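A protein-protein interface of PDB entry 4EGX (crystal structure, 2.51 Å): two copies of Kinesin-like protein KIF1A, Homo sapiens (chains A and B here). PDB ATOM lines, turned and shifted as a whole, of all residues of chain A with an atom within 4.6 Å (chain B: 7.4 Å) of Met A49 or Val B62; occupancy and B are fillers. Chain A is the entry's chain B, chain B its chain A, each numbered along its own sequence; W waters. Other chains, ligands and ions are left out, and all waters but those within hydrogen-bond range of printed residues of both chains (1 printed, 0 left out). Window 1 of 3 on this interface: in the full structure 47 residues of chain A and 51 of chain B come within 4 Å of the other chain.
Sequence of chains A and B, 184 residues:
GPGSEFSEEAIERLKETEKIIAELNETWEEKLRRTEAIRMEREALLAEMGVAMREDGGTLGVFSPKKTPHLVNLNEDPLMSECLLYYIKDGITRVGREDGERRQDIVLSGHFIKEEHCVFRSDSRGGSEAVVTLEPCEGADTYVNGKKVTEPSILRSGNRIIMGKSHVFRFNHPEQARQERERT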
ATOM      1  N   LEU A  45     -14.481 -12.910 -12.213  1.00  0.00           N
ATOM      2  CA  LEU A  45     -13.917 -14.262 -12.216  1.00  0.00           C
ATOM      3  C   LEU A  45     -14.066 -14.956 -13.572  1.00  0.00           C
ATOM      4  O   LEU A  45     -13.163 -15.673 -14.008  1.00  0.00           O
ATOM      5  CB  LEU A  45     -14.568 -15.125 -11.134  1.00  0.00           C
ATOM      6  CG  LEU A  45     -13.708 -16.148 -10.370  1.00  0.00           C
ATOM      7  CD1 LEU A  45     -14.591 -17.102  -9.581  1.00  0.00           C
ATOM      8  CD2 LEU A  45     -12.699 -16.929 -11.232  1.00  0.00           C
ATOM      9  N   ALA A  47     -13.615 -13.974 -16.332  1.00  0.00           N
ATOM     10  CA  ALA A  47     -12.449 -13.629 -17.133  1.00  0.00           C
ATOM     11  C   ALA A  47     -11.517 -12.724 -16.322  1.00  0.00           C
ATOM     12  O   ALA A  47     -11.300 -11.559 -16.683  1.00  0.00           O
ATOM     13  CB  ALA A  47     -12.887 -12.940 -18.428  1.00  0.00           C
ATOM     14  N   GLU A  48     -10.987 -13.250 -15.212  1.00  0.00           N
ATOM     15  CA  GLU A  48     -10.106 -12.457 -14.347  1.00  0.00           C
ATOM     16  C   GLU A  48      -8.675 -12.975 -14.360  1.00  0.00           C
ATOM     17  O   GLU A  48      -7.782 -12.320 -14.909  1.00  0.00           O
ATOM     18  CB  GLU A  48     -10.634 -12.380 -12.916  1.00  0.00           C
ATOM     19  CG  GLU A  48     -10.393 -11.025 -12.283  1.00  0.00           C
ATOM     20  CD  GLU A  48     -10.729 -10.987 -10.812  1.00  0.00           C
ATOM     21  OE1 GLU A  48     -10.295 -10.017 -10.146  1.00  0.00           O
ATOM     22  OE2 GLU A  48     -11.419 -11.918 -10.323  1.00  0.00           O
ATOM     23  N   MET A  49      -8.447 -14.135 -13.742  1.00  0.00           N
ATOM     24  CA  MET A  49      -7.189 -14.837 -13.958  1.00  0.00           C
ATOM     25  C   MET A  49      -7.113 -15.135 -15.459  1.00  0.00           C
ATOM     26  O   MET A  49      -6.070 -14.908 -16.102  1.00  0.00           O
ATOM     27  CB  MET A  49      -7.066 -16.103 -13.097  1.00  0.00           C
ATOM     28  CG  MET A  49      -8.365 -16.869 -12.838  1.00  0.00           C
ATOM     29  SD  MET A  49      -8.133 -18.196 -11.623  1.00  0.00           S
ATOM     30  CE  MET A  49      -9.656 -19.105 -11.862  1.00  0.00           C
ATOM     31  N   GLY A  50      -8.235 -15.588 -16.020  1.00  0.00           N
ATOM     32  CA  GLY A  50      -8.378 -15.618 -17.463  1.00  0.00           C
ATOM     33  C   GLY A  50      -8.597 -16.987 -18.063  1.00  0.00           C
ATOM     34  O   GLY A  50      -8.356 -18.020 -17.420  1.00  0.00           O
ATOM     35  N   VAL A  62      -6.867 -22.295 -17.736  1.00  0.00           N
ATOM     36  CA  VAL A  62      -7.062 -21.392 -16.623  1.00  0.00           C
ATOM     37  C   VAL A  62      -5.712 -20.881 -16.166  1.00  0.00           C
ATOM     38  O   VAL A  62      -4.828 -21.660 -15.810  1.00  0.00           O
ATOM     39  CB  VAL A  62      -7.778 -22.067 -15.428  1.00  0.00           C
ATOM     40  CG1 VAL A  62      -8.091 -21.018 -14.385  1.00  0.00           C
ATOM     41  CG2 VAL A  62      -9.073 -22.781 -15.868  1.00  0.00           C
ATOM     42  N   PHE A  63      -5.540 -19.573 -16.196  1.00  0.00           N
ATOM     43  CA  PHE A  63      -4.374 -18.987 -15.581  1.00  0.00           C
ATOM     44  C   PHE A  63      -4.655 -18.915 -14.098  1.00  0.00           C
ATOM     45  O   PHE A  63      -5.809 -18.854 -13.700  1.00  0.00           O
ATOM     46  CB  PHE A  63      -4.097 -17.613 -16.167  1.00  0.00           C
ATOM     47  CG  PHE A  63      -3.797 -17.639 -17.639  1.00  0.00           C
ATOM     48  CD1 PHE A  63      -2.489 -17.805 -18.093  1.00  0.00           C
ATOM     49  CD2 PHE A  63      -4.825 -17.512 -18.575  1.00  0.00           C
ATOM     50  CE1 PHE A  63      -2.216 -17.831 -19.448  1.00  0.00           C
ATOM     51  CE2 PHE A  63      -4.553 -17.538 -19.930  1.00  0.00           C
ATOM     52  CZ  PHE A  63      -3.250 -17.695 -20.369  1.00  0.00           C
ATOM     53  N   SER A  64      -3.605 -18.999 -13.288  1.00  0.00           N
ATOM     54  CA  SER A  64      -3.733 -18.772 -11.853  1.00  0.00           C
ATOM     55  C   SER A  64      -3.813 -17.272 -11.642  1.00  0.00           C
ATOM     56  O   SER A  64      -3.282 -16.507 -12.460  1.00  0.00           O
ATOM     57  CB  SER A  64      -2.545 -19.366 -11.084  1.00  0.00           C
ATOM     58  OG  SER A  64      -1.297 -18.925 -11.605  1.00  0.00           O
ATOM     59  N   PRO A  65      -4.490 -16.837 -10.560  1.00  0.00           N
ATOM     60  CA  PRO A  65      -4.671 -15.415 -10.295  1.00  0.00           C
ATOM     61  C   PRO A  65      -3.352 -14.673 -10.367  1.00  0.00           C
ATOM     62  O   PRO A  65      -2.309 -15.227 -10.021  1.00  0.00           O
ATOM     63  CB  PRO A  65      -5.209 -15.400  -8.867  1.00  0.00           C
ATOM     64  CG  PRO A  65      -5.905 -16.676  -8.732  1.00  0.00           C
ATOM     65  CD  PRO A  65      -5.127 -17.666  -9.518  1.00  0.00           C
ATOM     66  N   LYS A  66      -3.399 -13.424 -10.811  1.00  0.00           N
ATOM     67  CA  LYS A  66      -2.171 -12.680 -11.073  1.00  0.00           C
ATOM     68  C   LYS A  66      -1.772 -11.751  -9.930  1.00  0.00           C
ATOM     69  O   LYS A  66      -0.634 -11.274  -9.893  1.00  0.00           O
ATOM     70  CB  LYS A  66      -2.274 -11.905 -12.391  1.00  0.00           C
ATOM     71  CG  LYS A  66      -2.817 -12.737 -13.545  1.00  0.00           C
ATOM     72  CD  LYS A  66      -2.272 -12.254 -14.903  1.00  0.00           C
ATOM     73  CE  LYS A  66      -3.153 -12.792 -16.030  1.00  0.00           C
ATOM     74  NZ  LYS A  66      -3.223 -14.312 -16.032  1.00  0.00           N
ATOM     75  N   CYS A  83     -10.473 -28.979  -4.714  1.00  0.00           N
ATOM     76  CA  CYS A  83     -10.130 -28.103  -5.808  1.00  0.00           C
ATOM     77  C   CYS A  83      -8.664 -28.211  -6.126  1.00  0.00           C
ATOM     78  O   CYS A  83      -7.845 -28.460  -5.241  1.00  0.00           O
ATOM     79  CB  CYS A  83     -10.443 -26.669  -5.444  1.00  0.00           C
ATOM     80  SG  CYS A  83     -12.161 -26.433  -5.224  1.00  0.00           S
ATOM     81  N   LEU A  84      -8.354 -28.021  -7.405  1.00  0.00           N
ATOM     82  CA  LEU A  84      -6.988 -27.892  -7.886  1.00  0.00           C
ATOM     83  C   LEU A  84      -6.384 -26.587  -7.357  1.00  0.00           C
ATOM     84  O   LEU A  84      -5.200 -26.526  -7.017  1.00  0.00           O
ATOM     85  CB  LEU A  84      -6.989 -27.932  -9.420  1.00  0.00           C
ATOM     86  CG  LEU A  84      -5.754 -27.622 -10.278  1.00  0.00           C
ATOM     87  CD1 LEU A  84      -5.762 -28.496 -11.516  1.00  0.00           C
ATOM     88  CD2 LEU A  84      -5.762 -26.162 -10.679  1.00  0.00           C
ATOM     89  N   LEU A  85      -7.208 -25.549  -7.286  1.00  0.00           N
ATOM     90  CA  LEU A  85      -6.757 -24.249  -6.820  1.00  0.00           C
ATOM     91  C   LEU A  85      -7.725 -23.709  -5.762  1.00  0.00           C
ATOM     92  O   LEU A  85      -8.928 -23.760  -5.950  1.00  0.00           O
ATOM     93  CB  LEU A  85      -6.607 -23.278  -8.002  1.00  0.00           C
ATOM     94  CG  LEU A  85      -5.734 -22.031  -7.816  1.00  0.00           C
ATOM     95  CD1 LEU A  85      -5.038 -21.669  -9.085  1.00  0.00           C
ATOM     96  CD2 LEU A  85      -6.553 -20.841  -7.313  1.00  0.00           C
ATOM     97  N   TYR A  87      -8.532 -20.230  -3.138  1.00  0.00           N
ATOM     98  CA  TYR A  87      -8.258 -18.819  -2.930  1.00  0.00           C
ATOM     99  C   TYR A  87      -8.023 -18.506  -1.475  1.00  0.00           C
ATOM    100  O   TYR A  87      -8.797 -18.934  -0.625  1.00  0.00           O
ATOM    101  CB  TYR A  87      -9.424 -17.982  -3.452  1.00  0.00           C
ATOM    102  CG  TYR A  87      -9.406 -17.857  -4.950  1.00  0.00           C
ATOM    103  CD1 TYR A  87      -8.557 -16.942  -5.569  1.00  0.00           C
ATOM    104  CD2 TYR A  87     -10.227 -18.655  -5.754  1.00  0.00           C
ATOM    105  CE1 TYR A  87      -8.529 -16.813  -6.937  1.00  0.00           C
ATOM    106  CE2 TYR A  87     -10.206 -18.536  -7.135  1.00  0.00           C
ATOM    107  CZ  TYR A  87      -9.345 -17.613  -7.722  1.00  0.00           C
ATOM    108  OH  TYR A  87      -9.291 -17.456  -9.091  1.00  0.00           O
ATOM    109  N   LEU B  46     -19.880 -20.395 -14.122  1.00  0.00           N
ATOM    110  CA  LEU B  46     -18.590 -20.625 -13.476  1.00  0.00           C
ATOM    111  C   LEU B  46     -18.358 -22.052 -12.983  1.00  0.00           C
ATOM    112  O   LEU B  46     -17.224 -22.548 -13.020  1.00  0.00           O
ATOM    113  CB  LEU B  46     -18.339 -19.600 -12.379  1.00  0.00           C
ATOM    114  CG  LEU B  46     -17.882 -18.306 -13.038  1.00  0.00           C
ATOM    115  CD1 LEU B  46     -17.535 -17.262 -12.002  1.00  0.00           C
ATOM    116  CD2 LEU B  46     -16.674 -18.618 -13.903  1.00  0.00           C
ATOM    117  N   MET B  49     -17.472 -23.919 -15.925  1.00  0.00           N
ATOM    118  CA  MET B  49     -16.076 -23.601 -16.234  1.00  0.00           C
ATOM    119  C   MET B  49     -15.089 -24.202 -15.206  1.00  0.00           C
ATOM    120  O   MET B  49     -13.866 -24.142 -15.388  1.00  0.00           O
ATOM    121  CB  MET B  49     -15.903 -22.087 -16.447  1.00  0.00           C
ATOM    122  CG  MET B  49     -16.621 -21.611 -17.716  1.00  0.00           C
ATOM    123  SD  MET B  49     -16.782 -19.827 -17.996  1.00  0.00           S
ATOM    124  CE  MET B  49     -15.238 -19.471 -18.833  1.00  0.00           C
ATOM    125  N   GLY B  50     -15.639 -24.800 -14.145  1.00  0.00           N
ATOM    126  CA  GLY B  50     -14.848 -25.537 -13.154  1.00  0.00           C
ATOM    127  C   GLY B  50     -14.468 -24.789 -11.880  1.00  0.00           C
ATOM    128  O   GLY B  50     -13.511 -25.161 -11.194  1.00  0.00           O
ATOM    129  N   VAL B  51     -15.205 -23.730 -11.562  1.00  0.00           N
ATOM    130  CA  VAL B  51     -14.991 -23.014 -10.318  1.00  0.00           C
ATOM    131  C   VAL B  51     -15.802 -23.715  -9.239  1.00  0.00           C
ATOM    132  O   VAL B  51     -16.879 -24.256  -9.526  1.00  0.00           O
ATOM    133  CB  VAL B  51     -15.396 -21.524 -10.439  1.00  0.00           C
ATOM    134  CG1 VAL B  51     -15.307 -20.812  -9.084  1.00  0.00           C
ATOM    135  CG2 VAL B  51     -14.517 -20.823 -11.486  1.00  0.00           C
ATOM    136  N   ALA B  52     -15.270 -23.723  -8.013  1.00  0.00           N
ATOM    137  CA  ALA B  52     -15.981 -24.256  -6.848  1.00  0.00           C
ATOM    138  C   ALA B  52     -16.638 -23.139  -6.047  1.00  0.00           C
ATOM    139  O   ALA B  52     -16.004 -22.140  -5.722  1.00  0.00           O
ATOM    140  CB  ALA B  52     -15.047 -25.045  -5.966  1.00  0.00           C
ATOM    141  N   LEU B  60     -14.618 -20.279  -4.201  1.00  0.00           N
ATOM    142  CA  LEU B  60     -13.728 -21.073  -3.348  1.00  0.00           C
ATOM    143  C   LEU B  60     -12.441 -21.463  -4.071  1.00  0.00           C
ATOM    144  O   LEU B  60     -11.373 -21.527  -3.456  1.00  0.00           O
ATOM    145  CB  LEU B  60     -14.438 -22.347  -2.851  1.00  0.00           C
ATOM    146  CG  LEU B  60     -15.750 -22.157  -2.045  1.00  0.00           C
ATOM    147  CD1 LEU B  60     -16.310 -23.494  -1.622  1.00  0.00           C
ATOM    148  CD2 LEU B  60     -15.515 -21.277  -0.827  1.00  0.00           C
ATOM    149  N   GLY B  61     -12.549 -21.729  -5.370  1.00  0.00           N
ATOM    150  CA  GLY B  61     -11.393 -22.136  -6.168  1.00  0.00           C
ATOM    151  C   GLY B  61     -11.733 -22.956  -7.402  1.00  0.00           C
ATOM    152  O   GLY B  61     -12.873 -22.925  -7.877  1.00  0.00           O
ATOM    153  N   VAL B  62     -10.739 -23.681  -7.924  1.00  0.00           N
ATOM    154  CA  VAL B  62     -10.869 -24.397  -9.202  1.00  0.00           C
ATOM    155  C   VAL B  62     -10.602 -25.892  -9.072  1.00  0.00           C
ATOM    156  O   VAL B  62      -9.561 -26.303  -8.584  1.00  0.00           O
ATOM    157  CB  VAL B  62      -9.920 -23.838 -10.289  1.00  0.00           C
ATOM    158  CG1 VAL B  62     -10.400 -24.258 -11.673  1.00  0.00           C
ATOM    159  CG2 VAL B  62      -9.815 -22.329 -10.198  1.00  0.00           C
ATOM    160  N   PHE B  63     -11.564 -26.688  -9.526  1.00  0.00           N
ATOM    161  CA  PHE B  63     -11.443 -28.134  -9.549  1.00  0.00           C
ATOM    162  C   PHE B  63     -10.574 -28.607 -10.688  1.00  0.00           C
ATOM    163  O   PHE B  63     -10.480 -27.966 -11.727  1.00  0.00           O
ATOM    164  CB  PHE B  63     -12.817 -28.778  -9.733  1.00  0.00           C
ATOM    165  CG  PHE B  63     -13.706 -28.693  -8.519  1.00  0.00           C
ATOM    166  CD1 PHE B  63     -13.366 -29.349  -7.333  1.00  0.00           C
ATOM    167  CD2 PHE B  63     -14.906 -27.981  -8.572  1.00  0.00           C
ATOM    168  CE1 PHE B  63     -14.204 -29.284  -6.220  1.00  0.00           C
ATOM    169  CE2 PHE B  63     -15.743 -27.917  -7.464  1.00  0.00           C
ATOM    170  CZ  PHE B  63     -15.388 -28.570  -6.287  1.00  0.00           C
ATOM    171  N   SER B  64      -9.940 -29.754 -10.489  1.00  0.00           N
ATOM    172  CA  SER B  64      -9.409 -30.516 -11.609  1.00  0.00           C
ATOM    173  C   SER B  64     -10.631 -31.095 -12.324  1.00  0.00           C
ATOM    174  O   SER B  64     -11.647 -31.376 -11.676  1.00  0.00           O
ATOM    175  CB  SER B  64      -8.483 -31.624 -11.116  1.00  0.00           C
ATOM    176  OG  SER B  64      -7.326 -31.695 -11.933  1.00  0.00           O
ATOM    177  N   PRO B  65     -10.573 -31.225 -13.662  1.00  0.00           N
ATOM    178  CA  PRO B  65     -11.682 -31.867 -14.373  1.00  0.00           C
ATOM    179  C   PRO B  65     -11.816 -33.359 -14.052  1.00  0.00           C
ATOM    180  O   PRO B  65     -10.817 -34.037 -13.799  1.00  0.00           O
ATOM    181  CB  PRO B  65     -11.321 -31.665 -15.848  1.00  0.00           C
ATOM    182  CG  PRO B  65     -10.329 -30.581 -15.862  1.00  0.00           C
ATOM    183  CD  PRO B  65      -9.542 -30.755 -14.595  1.00  0.00           C
ATOM    184  N   LEU B  84      -2.192 -22.620 -15.599  1.00  0.00           N
ATOM    185  CA  LEU B  84      -2.099 -23.655 -14.601  1.00  0.00           C
ATOM    186  C   LEU B  84      -2.750 -24.937 -15.132  1.00  0.00           C
ATOM    187  O   LEU B  84      -2.221 -26.032 -14.950  1.00  0.00           O
ATOM    188  CB  LEU B  84      -2.758 -23.224 -13.298  1.00  0.00           C
ATOM    189  CG  LEU B  84      -2.527 -24.267 -12.211  1.00  0.00           C
ATOM    190  CD1 LEU B  84      -1.096 -24.144 -11.699  1.00  0.00           C
ATOM    191  CD2 LEU B  84      -3.526 -24.067 -11.099  1.00  0.00           C
ATOM    192  N   LEU B  85      -3.890 -24.802 -15.797  1.00  0.00           N
ATOM    193  CA  LEU B  85      -4.565 -25.964 -16.368  1.00  0.00           C
ATOM    194  C   LEU B  85      -4.833 -25.748 -17.849  1.00  0.00           C
ATOM    195  O   LEU B  85      -5.340 -24.701 -18.229  1.00  0.00           O
ATOM    196  CB  LEU B  85      -5.884 -26.177 -15.635  1.00  0.00           C
ATOM    197  CG  LEU B  85      -6.579 -27.530 -15.730  1.00  0.00           C
ATOM    198  CD1 LEU B  85      -5.600 -28.610 -15.381  1.00  0.00           C
ATOM    199  CD2 LEU B  85      -7.774 -27.559 -14.786  1.00  0.00           C
ATOM    200  N   TYR B  87      -6.861 -27.723 -21.079  1.00  0.00           N
ATOM    201  CA  TYR B  87      -7.743 -28.826 -21.357  1.00  0.00           C
ATOM    202  C   TYR B  87      -7.308 -29.429 -22.667  1.00  0.00           C
ATOM    203  O   TYR B  87      -6.655 -28.760 -23.478  1.00  0.00           O
ATOM    204  CB  TYR B  87      -9.191 -28.360 -21.432  1.00  0.00           C
ATOM    205  CG  TYR B  87      -9.664 -27.628 -20.202  1.00  0.00           C
ATOM    206  CD1 TYR B  87      -9.514 -28.174 -18.933  1.00  0.00           C
ATOM    207  CD2 TYR B  87     -10.274 -26.390 -20.312  1.00  0.00           C
ATOM    208  CE1 TYR B  87      -9.953 -27.491 -17.805  1.00  0.00           C
ATOM    209  CE2 TYR B  87     -10.723 -25.703 -19.192  1.00  0.00           C
ATOM    210  CZ  TYR B  87     -10.560 -26.256 -17.946  1.00  0.00           C
ATOM    211  OH  TYR B  87     -11.013 -25.554 -16.845  1.00  0.00           O
HETATM  212  O   HOH W   1     -12.164 -19.577  -0.758  1.00  0.00           O
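N of Leu A84 is in hydrogen-bond range of O of Val B62 (2.4 Å). The backbone carbonyl oxygen (O) of Leu B85 sits at hydrogen-bond distance from the backbone NH (N) of Val A62, at 2.9 Å. The backbone NH (N) of Val B62 sits at hydrogen-bond distance from the backbone carbonyl oxygen (O) of Leu A85, at 2.7 Å. The backbone NH (N) of Leu B84 lies within hydrogen-bond range of the backbone carbonyl oxygen (O) of Val A62 (2.8 Å). O of Leu B60 sits at hydrogen-bond distance from N of Tyr A87, 3.1 Å away.
The side-chain hydroxyl (OH) of Tyr A87 is in hydrogen-bond range of the side-chain sulfur (SD) of Met A49 (2.9 Å). The backbone NH (N) of Phe B63 lies within hydrogen-bond range of the backbone carbonyl oxygen (O) of Gly B50 (3.0 Å). The backbone NH of Ala B52 lies within hydrogen-bond range of the backbone carbonyl oxygen of Gly B61 (2.5 Å). O of Ala B52 lies within hydrogen-bond range of N of Leu B60. NZ of Lys A66 lies within hydrogen-bond range of O of Met A49 (2.9 Å). The backbone carbonyl oxygen of Leu B46 lies within hydrogen-bond range of the backbone NH of Val B51 (2.8 Å).
CD1 of Leu A45 touches CG1 of Val B51 (3.8 Å). CE of Met A49 touches CG2 of Val B62 (3.6 Å). Val A62 touches Tyr B87. Cys A83 touches Ala B52. CE1 of Phe B63 touches SG of Cys A83, 3.6 Å away. Leu A84 touches Phe B63. Ser B64 touches Leu A84. Leu B84 touches Leu A84 (CD2 to CD2, 3.1 Å). Leu A85 touches Gly B61. Gly B61 touches Tyr A87 (CA to CD2, 3.7 Å).
Glu A48 touches none of the printed residues of chain B. Met A49 touches one residue of chain B. Pro A65 touches none of the printed residues of chain B. Of the printed residues of chain B, Tyr A87 touches Leu B60 (3.1 Å) and Gly B61 (3.7 Å). Printed residues of chain A within 4 Å of Val B51: Leu A45. Of the printed residues of chain A, Val B62 touches Met A49, Cys A83, Leu A84 and Leu A85. Of the printed residues of chain A, Phe B63 touches Cys A83 and Leu A84. The nearest residue of chain B that does not touch Met A49 is Val B51 (5.2 Å). The nearest printed residue of chain A that does not touch Val B62 is Val A62 (4.6 Å). The nearest printed residue of chain A that does not touch Gly B61 is Cys A83 (4.1 Å).
Printed residues of chain B that touch a printed residue of chain A: Leu B46, Val B51, Ala B52, Leu B60, Gly B61, Val B62, Phe B63, Ser B64, Leu B84, Leu B85 and Tyr B87. Among the printed residues, no Asp or Glu carboxylate lies within 4 Å of a Lys or Arg side-chain nitrogen of the other chain.
Val A62 touches Leu B84, and with the chains exchanged Leu A84 touches Val B62. Val A62 touches Tyr B87, but with the chains exchanged Tyr A87 does not touch Val B62 (4.9 Å). Leu A84 touches Ser B64, but with the chains exchanged Ser A64 does not touch Leu B84 (4.3 Å). Leu A84 touches Leu B85, and with the chains exchanged Leu A85 touches Leu B84. Of the 19 pairs that touch across the chains among the printed residues, 7 have their exchanged pair printed and touching as well.
Water W1 lies within hydrogen-bond range of O of Leu B60 (3.4 Å) and O of Tyr A87 (3.4 Å).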
